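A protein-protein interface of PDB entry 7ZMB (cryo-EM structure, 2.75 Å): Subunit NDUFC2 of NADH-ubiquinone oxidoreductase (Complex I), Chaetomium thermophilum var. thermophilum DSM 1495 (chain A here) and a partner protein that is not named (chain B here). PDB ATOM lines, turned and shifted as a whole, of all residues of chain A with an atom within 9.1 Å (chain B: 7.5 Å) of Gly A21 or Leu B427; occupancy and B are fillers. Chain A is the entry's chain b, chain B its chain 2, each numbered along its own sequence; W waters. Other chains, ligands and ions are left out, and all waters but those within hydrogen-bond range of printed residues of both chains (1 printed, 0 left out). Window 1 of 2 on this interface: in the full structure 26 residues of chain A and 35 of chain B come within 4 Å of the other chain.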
ATOM      1  N   ALA A  14      12.262   4.064 -32.002  1.00  0.00           N
ATOM      2  CA  ALA A  14      12.444   4.653 -30.684  1.00  0.00           C
ATOM      3  C   ALA A  14      12.711   3.615 -29.603  1.00  0.00           C
ATOM      4  O   ALA A  14      13.340   3.948 -28.595  1.00  0.00           O
ATOM      5  CB  ALA A  14      11.226   5.493 -30.306  1.00  0.00           C
ATOM      6  N   VAL A  15      12.242   2.380 -29.770  1.00  0.00           N
ATOM      7  CA  VAL A  15      12.616   1.334 -28.827  1.00  0.00           C
ATOM      8  C   VAL A  15      14.119   1.092 -28.879  1.00  0.00           C
ATOM      9  O   VAL A  15      14.782   0.988 -27.843  1.00  0.00           O
ATOM     10  CB  VAL A  15      11.825   0.045 -29.101  1.00  0.00           C
ATOM     11  CG1 VAL A  15      12.315  -1.072 -28.199  1.00  0.00           C
ATOM     12  CG2 VAL A  15      10.340   0.275 -28.919  1.00  0.00           C
ATOM     13  N   ARG A  16      14.678   1.013 -30.084  1.00  0.00           N
ATOM     14  CA  ARG A  16      16.116   0.833 -30.230  1.00  0.00           C
ATOM     15  C   ARG A  16      16.879   2.020 -29.656  1.00  0.00           C
ATOM     16  O   ARG A  16      17.931   1.848 -29.035  1.00  0.00           O
ATOM     17  CB  ARG A  16      16.451   0.618 -31.703  1.00  0.00           C
ATOM     18  CG  ARG A  16      17.886   0.248 -32.007  1.00  0.00           C
ATOM     19  CD  ARG A  16      18.363  -0.988 -31.293  1.00  0.00           C
ATOM     20  NE  ARG A  16      19.806  -1.112 -31.436  1.00  0.00           N
ATOM     21  CZ  ARG A  16      20.530  -2.135 -31.001  1.00  0.00           C
ATOM     22  NH1 ARG A  16      21.838  -2.141 -31.191  1.00  0.00           N
ATOM     23  NH2 ARG A  16      19.953  -3.141 -30.378  1.00  0.00           N
ATOM     24  N   PHE A  17      16.358   3.231 -29.850  1.00  0.00           N
ATOM     25  CA  PHE A  17      16.968   4.411 -29.245  1.00  0.00           C
ATOM     26  C   PHE A  17      16.920   4.335 -27.728  1.00  0.00           C
ATOM     27  O   PHE A  17      17.930   4.544 -27.049  1.00  0.00           O
ATOM     28  CB  PHE A  17      16.254   5.667 -29.728  1.00  0.00           C
ATOM     29  CG  PHE A  17      17.123   6.877 -29.755  1.00  0.00           C
ATOM     30  CD1 PHE A  17      18.302   6.878 -30.485  1.00  0.00           C
ATOM     31  CD2 PHE A  17      16.782   8.005 -29.036  1.00  0.00           C
ATOM     32  CE1 PHE A  17      19.110   7.990 -30.514  1.00  0.00           C
ATOM     33  CE2 PHE A  17      17.588   9.117 -29.060  1.00  0.00           C
ATOM     34  CZ  PHE A  17      18.757   9.109 -29.797  1.00  0.00           C
ATOM     35  N   TRP A  18      15.745   4.031 -27.175  1.00  0.00           N
ATOM     36  CA  TRP A  18      15.610   3.983 -25.727  1.00  0.00           C
ATOM     37  C   TRP A  18      16.399   2.824 -25.143  1.00  0.00           C
ATOM     38  O   TRP A  18      16.929   2.927 -24.033  1.00  0.00           O
ATOM     39  CB  TRP A  18      14.138   3.891 -25.346  1.00  0.00           C
ATOM     40  CG  TRP A  18      13.494   5.218 -25.150  1.00  0.00           C
ATOM     41  CD1 TRP A  18      13.056   6.065 -26.123  1.00  0.00           C
ATOM     42  CD2 TRP A  18      13.211   5.857 -23.905  1.00  0.00           C
ATOM     43  NE1 TRP A  18      12.521   7.196 -25.560  1.00  0.00           N
ATOM     44  CE2 TRP A  18      12.600   7.091 -24.199  1.00  0.00           C
ATOM     45  CE3 TRP A  18      13.411   5.509 -22.570  1.00  0.00           C
ATOM     46  CZ2 TRP A  18      12.194   7.974 -23.207  1.00  0.00           C
ATOM     47  CZ3 TRP A  18      13.011   6.389 -21.594  1.00  0.00           C
ATOM     48  CH2 TRP A  18      12.406   7.603 -21.914  1.00  0.00           C
ATOM     49  N   GLN A  19      16.496   1.717 -25.882  1.00  0.00           N
ATOM     50  CA  GLN A  19      17.327   0.602 -25.444  1.00  0.00           C
ATOM     51  C   GLN A  19      18.761   1.039 -25.221  1.00  0.00           C
ATOM     52  O   GLN A  19      19.349   0.779 -24.166  1.00  0.00           O
ATOM     53  CB  GLN A  19      17.329  -0.504 -26.483  1.00  0.00           C
ATOM     54  CG  GLN A  19      18.156  -1.675 -26.035  1.00  0.00           C
ATOM     55  CD  GLN A  19      18.208  -2.756 -27.053  1.00  0.00           C
ATOM     56  OE1 GLN A  19      17.654  -2.626 -28.135  1.00  0.00           O
ATOM     57  NE2 GLN A  19      18.893  -3.839 -26.726  1.00  0.00           N
ATOM     58  N   LEU A  20      19.351   1.676 -26.230  1.00  0.00           N
ATOM     59  CA  LEU A  20      20.759   2.033 -26.164  1.00  0.00           C
ATOM     60  C   LEU A  20      20.997   3.093 -25.101  1.00  0.00           C
ATOM     61  O   LEU A  20      22.038   3.089 -24.434  1.00  0.00           O
ATOM     62  CB  LEU A  20      21.231   2.502 -27.537  1.00  0.00           C
ATOM     63  CG  LEU A  20      21.096   1.450 -28.643  1.00  0.00           C
ATOM     64  CD1 LEU A  20      21.426   2.014 -30.012  1.00  0.00           C
ATOM     65  CD2 LEU A  20      21.947   0.234 -28.337  1.00  0.00           C
ATOM     66  N   GLY A  21      20.017   3.970 -24.916  1.00  0.00           N
ATOM     67  CA  GLY A  21      20.128   4.981 -23.854  1.00  0.00           C
ATOM     68  C   GLY A  21      20.110   4.324 -22.495  1.00  0.00           C
ATOM     69  O   GLY A  21      20.988   4.652 -21.679  1.00  0.00           O
ATOM     70  N   ILE A  22      19.138   3.442 -22.243  1.00  0.00           N
ATOM     71  CA  ILE A  22      19.105   2.700 -20.946  1.00  0.00           C
ATOM     72  C   ILE A  22      20.400   1.897 -20.793  1.00  0.00           C
ATOM     73  O   ILE A  22      20.978   1.928 -19.707  1.00  0.00           O
ATOM     74  CB  ILE A  22      17.854   1.803 -20.850  1.00  0.00           C
ATOM     75  CG1 ILE A  22      16.606   2.613 -20.498  1.00  0.00           C
ATOM     76  CG2 ILE A  22      18.060   0.642 -19.890  1.00  0.00           C
ATOM     77  CD1 ILE A  22      15.318   1.884 -20.770  1.00  0.00           C
ATOM     78  N   GLU A  23      20.873   1.248 -21.850  1.00  0.00           N
ATOM     79  CA  GLU A  23      22.093   0.407 -21.769  1.00  0.00           C
ATOM     80  C   GLU A  23      23.317   1.314 -21.707  1.00  0.00           C
ATOM     81  O   GLU A  23      24.408   0.799 -21.410  1.00  0.00           O
ATOM     82  CB  GLU A  23      22.178  -0.521 -22.977  1.00  0.00           C
ATOM     83  CG  GLU A  23      21.525  -1.867 -22.754  1.00  0.00           C
ATOM     84  CD  GLU A  23      21.554  -2.756 -23.983  1.00  0.00           C
ATOM     85  OE1 GLU A  23      21.353  -3.974 -23.833  1.00  0.00           O
ATOM     86  OE2 GLU A  23      21.776  -2.224 -25.088  1.00  0.00           O
ATOM     87  N   MET A  24      23.144   2.604 -21.985  1.00  0.00           N
ATOM     88  CA  MET A  24      24.278   3.564 -22.051  1.00  0.00           C
ATOM     89  C   MET A  24      25.264   3.127 -23.130  1.00  0.00           C
ATOM     90  O   MET A  24      26.481   3.246 -22.910  1.00  0.00           O
ATOM     91  CB  MET A  24      24.931   3.805 -20.693  1.00  0.00           C
ATOM     92  CG  MET A  24      24.029   4.598 -19.767  1.00  0.00           C
ATOM     93  SD  MET A  24      24.778   4.987 -18.177  1.00  0.00           S
ATOM     94  CE  MET A  24      25.168   3.343 -17.583  1.00  0.00           C
ATOM     95  N   ARG A  25      24.739   2.647 -24.263  1.00  0.00           N
ATOM     96  CA  ARG A  25      25.604   2.266 -25.406  1.00  0.00           C
ATOM     97  C   ARG A  25      25.494   3.353 -26.488  1.00  0.00           C
ATOM     98  O   ARG A  25      24.399   3.920 -26.619  1.00  0.00           O
ATOM     99  CB  ARG A  25      25.215   0.894 -25.961  1.00  0.00           C
ATOM    100  CG  ARG A  25      25.739  -0.293 -25.170  1.00  0.00           C
ATOM    101  CD  ARG A  25      25.192  -1.549 -25.808  1.00  0.00           C
ATOM    102  NE  ARG A  25      25.105  -1.363 -27.245  1.00  0.00           N
ATOM    103  CZ  ARG A  25      24.521  -2.210 -28.079  1.00  0.00           C
ATOM    104  NH1 ARG A  25      24.494  -1.948 -29.374  1.00  0.00           N
ATOM    105  NH2 ARG A  25      23.964  -3.314 -27.618  1.00  0.00           N
ATOM    106  N   PRO A  26      26.535   3.669 -27.295  1.00  0.00           N
ATOM    107  CA  PRO A  26      26.457   4.775 -28.256  1.00  0.00           C
ATOM    108  C   PRO A  26      25.364   4.542 -29.288  1.00  0.00           C
ATOM    109  O   PRO A  26      25.269   3.466 -29.882  1.00  0.00           O
ATOM    110  CB  PRO A  26      27.848   4.778 -28.901  1.00  0.00           C
ATOM    111  CG  PRO A  26      28.345   3.393 -28.706  1.00  0.00           C
ATOM    112  CD  PRO A  26      27.824   2.968 -27.380  1.00  0.00           C
ATOM    113  N   PHE A  27      24.536   5.558 -29.495  1.00  0.00           N
ATOM    114  CA  PHE A  27      23.613   5.515 -30.616  1.00  0.00           C
ATOM    115  C   PHE A  27      24.408   5.572 -31.913  1.00  0.00           C
ATOM    116  O   PHE A  27      25.477   6.184 -31.985  1.00  0.00           O
ATOM    117  CB  PHE A  27      22.642   6.694 -30.581  1.00  0.00           C
ATOM    118  CG  PHE A  27      21.968   6.907 -29.265  1.00  0.00           C
ATOM    119  CD1 PHE A  27      21.055   6.000 -28.777  1.00  0.00           C
ATOM    120  CD2 PHE A  27      22.206   8.056 -28.541  1.00  0.00           C
ATOM    121  CE1 PHE A  27      20.421   6.220 -27.571  1.00  0.00           C
ATOM    122  CE2 PHE A  27      21.580   8.279 -27.341  1.00  0.00           C
ATOM    123  CZ  PHE A  27      20.680   7.361 -26.858  1.00  0.00           C
ATOM    124  N   PHE A  28      23.887   4.914 -32.940  1.00  0.00           N
ATOM    125  CA  PHE A  28      24.399   5.047 -34.302  1.00  0.00           C
ATOM    126  C   PHE A  28      25.824   4.529 -34.444  1.00  0.00           C
ATOM    127  O   PHE A  28      26.588   5.008 -35.281  1.00  0.00           O
ATOM    128  CB  PHE A  28      24.296   6.494 -34.779  1.00  0.00           C
ATOM    129  CG  PHE A  28      22.916   7.061 -34.666  1.00  0.00           C
ATOM    130  CD1 PHE A  28      21.809   6.258 -34.851  1.00  0.00           C
ATOM    131  CD2 PHE A  28      22.724   8.393 -34.383  1.00  0.00           C
ATOM    132  CE1 PHE A  28      20.539   6.777 -34.752  1.00  0.00           C
ATOM    133  CE2 PHE A  28      21.458   8.914 -34.292  1.00  0.00           C
ATOM    134  CZ  PHE A  28      20.366   8.103 -34.478  1.00  0.00           C
ATOM    135  N   TYR A  36      18.219  -0.784 -36.612  1.00  0.00           N
ATOM    136  CA  TYR A  36      17.184   0.217 -36.789  1.00  0.00           C
ATOM    137  C   TYR A  36      16.216  -0.206 -37.889  1.00  0.00           C
ATOM    138  O   TYR A  36      15.001  -0.063 -37.719  1.00  0.00           O
ATOM    139  CB  TYR A  36      17.811   1.584 -37.062  1.00  0.00           C
ATOM    140  CG  TYR A  36      18.354   2.225 -35.807  1.00  0.00           C
ATOM    141  CD1 TYR A  36      17.511   2.871 -34.925  1.00  0.00           C
ATOM    142  CD2 TYR A  36      19.702   2.159 -35.495  1.00  0.00           C
ATOM    143  CE1 TYR A  36      17.989   3.446 -33.774  1.00  0.00           C
ATOM    144  CE2 TYR A  36      20.192   2.735 -34.340  1.00  0.00           C
ATOM    145  CZ  TYR A  36      19.325   3.380 -33.482  1.00  0.00           C
ATOM    146  OH  TYR A  36      19.783   3.961 -32.327  1.00  0.00           O
ATOM    147  N   ILE B 383      12.585  -1.974 -13.958  1.00  0.00           N
ATOM    148  CA  ILE B 383      13.497  -0.861 -13.714  1.00  0.00           C
ATOM    149  C   ILE B 383      14.183  -1.035 -12.368  1.00  0.00           C
ATOM    150  O   ILE B 383      15.402  -0.885 -12.253  1.00  0.00           O
ATOM    151  CB  ILE B 383      12.762   0.489 -13.806  1.00  0.00           C
ATOM    152  CG1 ILE B 383      12.203   0.719 -15.213  1.00  0.00           C
ATOM    153  CG2 ILE B 383      13.688   1.615 -13.424  1.00  0.00           C
ATOM    154  CD1 ILE B 383      10.898   1.492 -15.242  1.00  0.00           C
ATOM    155  N   TYR B 421      20.198   8.806  -9.107  1.00  0.00           N
ATOM    156  CA  TYR B 421      20.353   7.725 -10.107  1.00  0.00           C
ATOM    157  C   TYR B 421      20.337   8.332 -11.504  1.00  0.00           C
ATOM    158  O   TYR B 421      20.786   7.680 -12.454  1.00  0.00           O
ATOM    159  CB  TYR B 421      19.368   6.565  -9.935  1.00  0.00           C
ATOM    160  CG  TYR B 421      19.778   5.367 -10.755  1.00  0.00           C
ATOM    161  CD1 TYR B 421      20.867   4.594 -10.391  1.00  0.00           C
ATOM    162  CD2 TYR B 421      19.129   5.052 -11.936  1.00  0.00           C
ATOM    163  CE1 TYR B 421      21.275   3.517 -11.157  1.00  0.00           C
ATOM    164  CE2 TYR B 421      19.530   3.987 -12.721  1.00  0.00           C
ATOM    165  CZ  TYR B 421      20.601   3.211 -12.325  1.00  0.00           C
ATOM    166  OH  TYR B 421      20.985   2.152 -13.090  1.00  0.00           O
ATOM    167  N   PHE B 422      19.904   9.585 -11.601  1.00  0.00           N
ATOM    168  CA  PHE B 422      19.788  10.211 -12.929  1.00  0.00           C
ATOM    169  C   PHE B 422      21.195  10.618 -13.338  1.00  0.00           C
ATOM    170  O   PHE B 422      21.449  10.775 -14.538  1.00  0.00           O
ATOM    171  CB  PHE B 422      18.815  11.392 -12.862  1.00  0.00           C
ATOM    172  CG  PHE B 422      18.944  12.401 -13.972  1.00  0.00           C
ATOM    173  CD1 PHE B 422      18.435  12.133 -15.232  1.00  0.00           C
ATOM    174  CD2 PHE B 422      19.573  13.615 -13.757  1.00  0.00           C
ATOM    175  CE1 PHE B 422      18.556  13.059 -16.254  1.00  0.00           C
ATOM    176  CE2 PHE B 422      19.692  14.539 -14.781  1.00  0.00           C
ATOM    177  CZ  PHE B 422      19.181  14.259 -16.025  1.00  0.00           C
ATOM    178  N   ILE B 424      23.773   8.549 -12.727  1.00  0.00           N
ATOM    179  CA  ILE B 424      24.466   7.256 -12.998  1.00  0.00           C
ATOM    180  C   ILE B 424      23.953   6.737 -14.342  1.00  0.00           C
ATOM    181  O   ILE B 424      24.791   6.479 -15.214  1.00  0.00           O
ATOM    182  CB  ILE B 424      24.296   6.262 -11.834  1.00  0.00           C
ATOM    183  CG1 ILE B 424      24.996   6.767 -10.571  1.00  0.00           C
ATOM    184  CG2 ILE B 424      24.768   4.871 -12.224  1.00  0.00           C
ATOM    185  CD1 ILE B 424      24.711   5.947  -9.342  1.00  0.00           C
ATOM    186  N   ASN B 425      22.635   6.605 -14.501  1.00  0.00           N
ATOM    187  CA  ASN B 425      22.040   6.237 -15.813  1.00  0.00           C
ATOM    188  C   ASN B 425      20.799   7.105 -16.028  1.00  0.00           C
ATOM    189  O   ASN B 425      19.743   6.758 -15.473  1.00  0.00           O
ATOM    190  CB  ASN B 425      21.650   4.758 -15.869  1.00  0.00           C
ATOM    191  CG  ASN B 425      21.182   4.278 -17.224  1.00  0.00           C
ATOM    192  OD1 ASN B 425      20.810   5.061 -18.096  1.00  0.00           O
ATOM    193  ND2 ASN B 425      21.186   2.971 -17.402  1.00  0.00           N
ATOM    194  N   PRO B 426      20.866   8.164 -16.860  1.00  0.00           N
ATOM    195  CA  PRO B 426      19.726   9.066 -17.076  1.00  0.00           C
ATOM    196  C   PRO B 426      18.450   8.497 -17.728  1.00  0.00           C
ATOM    197  O   PRO B 426      17.396   8.853 -17.288  1.00  0.00           O
ATOM    198  CB  PRO B 426      20.338  10.177 -17.950  1.00  0.00           C
ATOM    199  CG  PRO B 426      21.507   9.526 -18.642  1.00  0.00           C
ATOM    200  CD  PRO B 426      22.054   8.554 -17.620  1.00  0.00           C
ATOM    201  N   LEU B 427      18.567   7.698 -18.791  1.00  0.00           N
ATOM    202  CA  LEU B 427      17.370   7.161 -19.502  1.00  0.00           C
ATOM    203  C   LEU B 427      16.620   6.132 -18.650  1.00  0.00           C
ATOM    204  O   LEU B 427      15.387   6.146 -18.690  1.00  0.00           O
ATOM    205  CB  LEU B 427      17.715   6.675 -20.911  1.00  0.00           C
ATOM    206  CG  LEU B 427      16.666   7.039 -21.959  1.00  0.00           C
ATOM    207  CD1 LEU B 427      16.195   8.471 -21.765  1.00  0.00           C
ATOM    208  CD2 LEU B 427      17.186   6.836 -23.371  1.00  0.00           C
ATOM    209  N   LEU B 428      17.283   5.297 -17.914  1.00  0.00           N
ATOM    210  CA  LEU B 428      16.610   4.329 -17.022  1.00  0.00           C
ATOM    211  C   LEU B 428      15.910   5.111 -15.910  1.00  0.00           C
ATOM    212  O   LEU B 428      14.875   4.641 -15.418  1.00  0.00           O
ATOM    213  CB  LEU B 428      17.682   3.372 -16.493  1.00  0.00           C
ATOM    214  CG  LEU B 428      17.187   2.143 -15.738  1.00  0.00           C
ATOM    215  CD1 LEU B 428      16.167   1.373 -16.562  1.00  0.00           C
ATOM    216  CD2 LEU B 428      18.355   1.247 -15.362  1.00  0.00           C
ATOM    217  N   SER B 429      16.483   6.277 -15.532  1.00  0.00           N
ATOM    218  CA  SER B 429      15.862   7.131 -14.492  1.00  0.00           C
ATOM    219  C   SER B 429      14.657   7.846 -15.092  1.00  0.00           C
ATOM    220  O   SER B 429      13.659   7.986 -14.387  1.00  0.00           O
ATOM    221  CB  SER B 429      16.867   8.108 -13.978  1.00  0.00           C
ATOM    222  OG  SER B 429      17.866   7.438 -13.238  1.00  0.00           O
ATOM    223  N   LEU B 430      14.748   8.260 -16.350  1.00  0.00           N
ATOM    224  CA  LEU B 430      13.585   8.829 -17.014  1.00  0.00           C
ATOM    225  C   LEU B 430      12.506   7.778 -17.247  1.00  0.00           C
ATOM    226  O   LEU B 430      11.315   8.081 -17.167  1.00  0.00           O
ATOM    227  CB  LEU B 430      14.010   9.469 -18.327  1.00  0.00           C
ATOM    228  CG  LEU B 430      12.993  10.419 -18.926  1.00  0.00           C
ATOM    229  CD1 LEU B 430      12.993  11.698 -18.149  1.00  0.00           C
ATOM    230  CD2 LEU B 430      13.341  10.664 -20.365  1.00  0.00           C
ATOM    231  N   SER B 431      12.902   6.540 -17.543  1.00  0.00           N
ATOM    232  CA  SER B 431      11.926   5.468 -17.696  1.00  0.00           C
ATOM    233  C   SER B 431      11.151   5.245 -16.407  1.00  0.00           C
ATOM    234  O   SER B 431       9.935   5.037 -16.434  1.00  0.00           O
ATOM    235  CB  SER B 431      12.625   4.183 -18.124  1.00  0.00           C
ATOM    236  OG  SER B 431      13.351   4.385 -19.315  1.00  0.00           O
ATOM    237  N   LEU B 432      11.839   5.275 -15.266  1.00  0.00           N
ATOM    238  CA  LEU B 432      11.152   5.124 -13.993  1.00  0.00           C
ATOM    239  C   LEU B 432      10.330   6.360 -13.650  1.00  0.00           C
ATOM    240  O   LEU B 432       9.269   6.242 -13.027  1.00  0.00           O
ATOM    241  CB  LEU B 432      12.168   4.804 -12.898  1.00  0.00           C
ATOM    242  CG  LEU B 432      11.653   4.540 -11.488  1.00  0.00           C
ATOM    243  CD1 LEU B 432      10.757   3.321 -11.464  1.00  0.00           C
ATOM    244  CD2 LEU B 432      12.828   4.310 -10.589  1.00  0.00           C
ATOM    245  N   ALA B 433      10.786   7.545 -14.060  1.00  0.00           N
ATOM    246  CA  ALA B 433       9.992   8.754 -13.872  1.00  0.00           C
ATOM    247  C   ALA B 433       8.681   8.683 -14.644  1.00  0.00           C
ATOM    248  O   ALA B 433       7.617   9.021 -14.113  1.00  0.00           O
ATOM    249  CB  ALA B 433      10.796   9.984 -14.291  1.00  0.00           C
ATOM    250  N   ILE B 434       8.734   8.237 -15.902  1.00  0.00           N
ATOM    251  CA  ILE B 434       7.522   8.153 -16.712  1.00  0.00           C
ATOM    252  C   ILE B 434       6.556   7.133 -16.123  1.00  0.00           C
ATOM    253  O   ILE B 434       5.341   7.358 -16.075  1.00  0.00           O
ATOM    254  CB  ILE B 434       7.876   7.823 -18.173  1.00  0.00           C
ATOM    255  CG1 ILE B 434       8.666   8.969 -18.804  1.00  0.00           C
ATOM    256  CG2 ILE B 434       6.627   7.520 -18.983  1.00  0.00           C
ATOM    257  CD1 ILE B 434       9.010   8.747 -20.245  1.00  0.00           C
ATOM    258  N   ILE B 532      23.907  -3.727 -19.335  1.00  0.00           N
ATOM    259  CA  ILE B 532      22.681  -4.521 -19.031  1.00  0.00           C
ATOM    260  C   ILE B 532      22.459  -5.461 -20.216  1.00  0.00           C
ATOM    261  O   ILE B 532      22.717  -5.039 -21.354  1.00  0.00           O
ATOM    262  CB  ILE B 532      21.495  -3.551 -18.877  1.00  0.00           C
ATOM    263  CG1 ILE B 532      21.773  -2.489 -17.810  1.00  0.00           C
ATOM    264  CG2 ILE B 532      20.193  -4.292 -18.616  1.00  0.00           C
ATOM    265  CD1 ILE B 532      20.974  -1.218 -17.980  1.00  0.00           C
ATOM    266  N   SER B 537      16.617  -4.342 -21.186  1.00  0.00           N
ATOM    267  CA  SER B 537      16.557  -2.980 -21.701  1.00  0.00           C
ATOM    268  C   SER B 537      15.520  -2.847 -22.813  1.00  0.00           C
ATOM    269  O   SER B 537      14.861  -1.810 -22.919  1.00  0.00           O
ATOM    270  CB  SER B 537      17.940  -2.533 -22.169  1.00  0.00           C
ATOM    271  OG  SER B 537      18.422  -3.344 -23.219  1.00  0.00           O
ATOM    272  N   ILE B 540      12.020  -2.867 -20.935  1.00  0.00           N
ATOM    273  CA  ILE B 540      11.755  -1.577 -20.309  1.00  0.00           C
ATOM    274  C   ILE B 540      11.480  -0.527 -21.373  1.00  0.00           C
ATOM    275  O   ILE B 540      10.630   0.351 -21.198  1.00  0.00           O
ATOM    276  CB  ILE B 540      12.925  -1.173 -19.396  1.00  0.00           C
ATOM    277  CG1 ILE B 540      13.046  -2.165 -18.239  1.00  0.00           C
ATOM    278  CG2 ILE B 540      12.719   0.228 -18.865  1.00  0.00           C
ATOM    279  CD1 ILE B 540      14.366  -2.151 -17.537  1.00  0.00           C
ATOM    280  N   THR B 544       7.925   1.537 -21.524  1.00  0.00           N
ATOM    281  CA  THR B 544       8.043   2.980 -21.362  1.00  0.00           C
ATOM    282  C   THR B 544       7.387   3.710 -22.525  1.00  0.00           C
ATOM    283  O   THR B 544       6.632   4.667 -22.328  1.00  0.00           O
ATOM    284  CB  THR B 544       9.511   3.387 -21.237  1.00  0.00           C
ATOM    285  OG1 THR B 544      10.146   2.577 -20.245  1.00  0.00           O
ATOM    286  CG2 THR B 544       9.628   4.843 -20.838  1.00  0.00           C
HETATM  287  O   HOH W   1      24.477  -0.694 -18.749  1.00  0.00           O
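Of the 16 printed residues of chain A, 6 touch a printed residue of chain B. Of the 18 printed residues of chain B, 11 touch a printed residue of chain A. Printed residues of chain B that touch a printed residue of chain A: Ile B424, Asn B425, Leu B427, Leu B428, Leu B430, Ser B431, Ile B434, Ile B532, Ser B537, Ile B540 and Thr B544.
The backbone carbonyl oxygen of Asn B425 is in hydrogen-bond range of the side-chain hydroxyl of Ser B429 (3.0 Å). The side-chain carboxylate (OE2) of Glu A23 is in salt-bridge range of the guanidinium group (NH2) of Arg A25 (3.5 Å). OE1 of Gln A19 is in hydrogen-bond range of NH2 of Arg A16, 3.3 Å away. OG1 of Thr B544 sits at hydrogen-bond distance from O of Ile B540. The side-chain hydroxyl of Ser B431 lies within hydrogen-bond range of the backbone carbonyl oxygen of Leu B427, 2.8 Å away.
Arg A16 touches none of the printed residues of chain B. Gly A21 touches two residues of chain B. Printed residues of chain A within 4 Å of Asn B425: Gly A21 (3.6 Å), Ile A22 (2.5 Å) and Met A24 (3.7 Å). No residue of chain A comes within 4 Å of Pro B426. Of chain A, only Trp A18 (3.6 Å), Gly A21 (3.5 Å) and Ile A22 (3.8 Å) come within 4 Å of Leu B427. Of the printed residues of chain A, Leu B428 touches Ile A22 (3.8 Å). Of the printed residues of chain A, Ser B431 touches Trp A18 and Ile A22. The nearest residue of chain B that does not touch Gly A21 is Leu B428 (5.3 Å). The nearest residue of chain A that does not touch Leu B427 is Phe A17 (4.4 Å). The nearest printed residue of chain B that does not touch Trp A18 is Ser B537 (5.3 Å).
The backbone carbonyl oxygen (O) of Ile B424 lies close to the side-chain sulfur (SD) of Met A24. The side-chain carboxylate of Glu A23 sits at hydrogen-bond distance from the side-chain hydroxyl of Ser B537 (3.1 Å). The side-chain carboxylate (OE1) of Glu A23 sits close to the backbone carbonyl oxygen (O) of Ile B532 (3.0 Å). The backbone carbonyl oxygen (O) of Ile A22 sits at hydrogen-bond distance from the side-chain amide nitrogen (ND2) of Asn B425, 2.5 Å away.
CE3 of Trp A18 touches CG of Leu B427, 3.6 Å away. Leu B430 touches Trp A18. Ser B431 touches Trp A18. Trp A18 touches Thr B544. Ser B537 touches Gln A19. Gly A21 touches Asn B425 (O to OD1, 3.6 Å). Ile A22 touches Leu B427. Ile A22 touches Ile B532. CB of Ser B537 touches CG2 of Ile A22 (3.9 Å). CG2 of Ile B540 touches CD1 of Ile A22 (3.6 Å).
Water W1 bridges O of Glu A23 (3.1 Å) and N of Ile B532 (3.1 Å).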
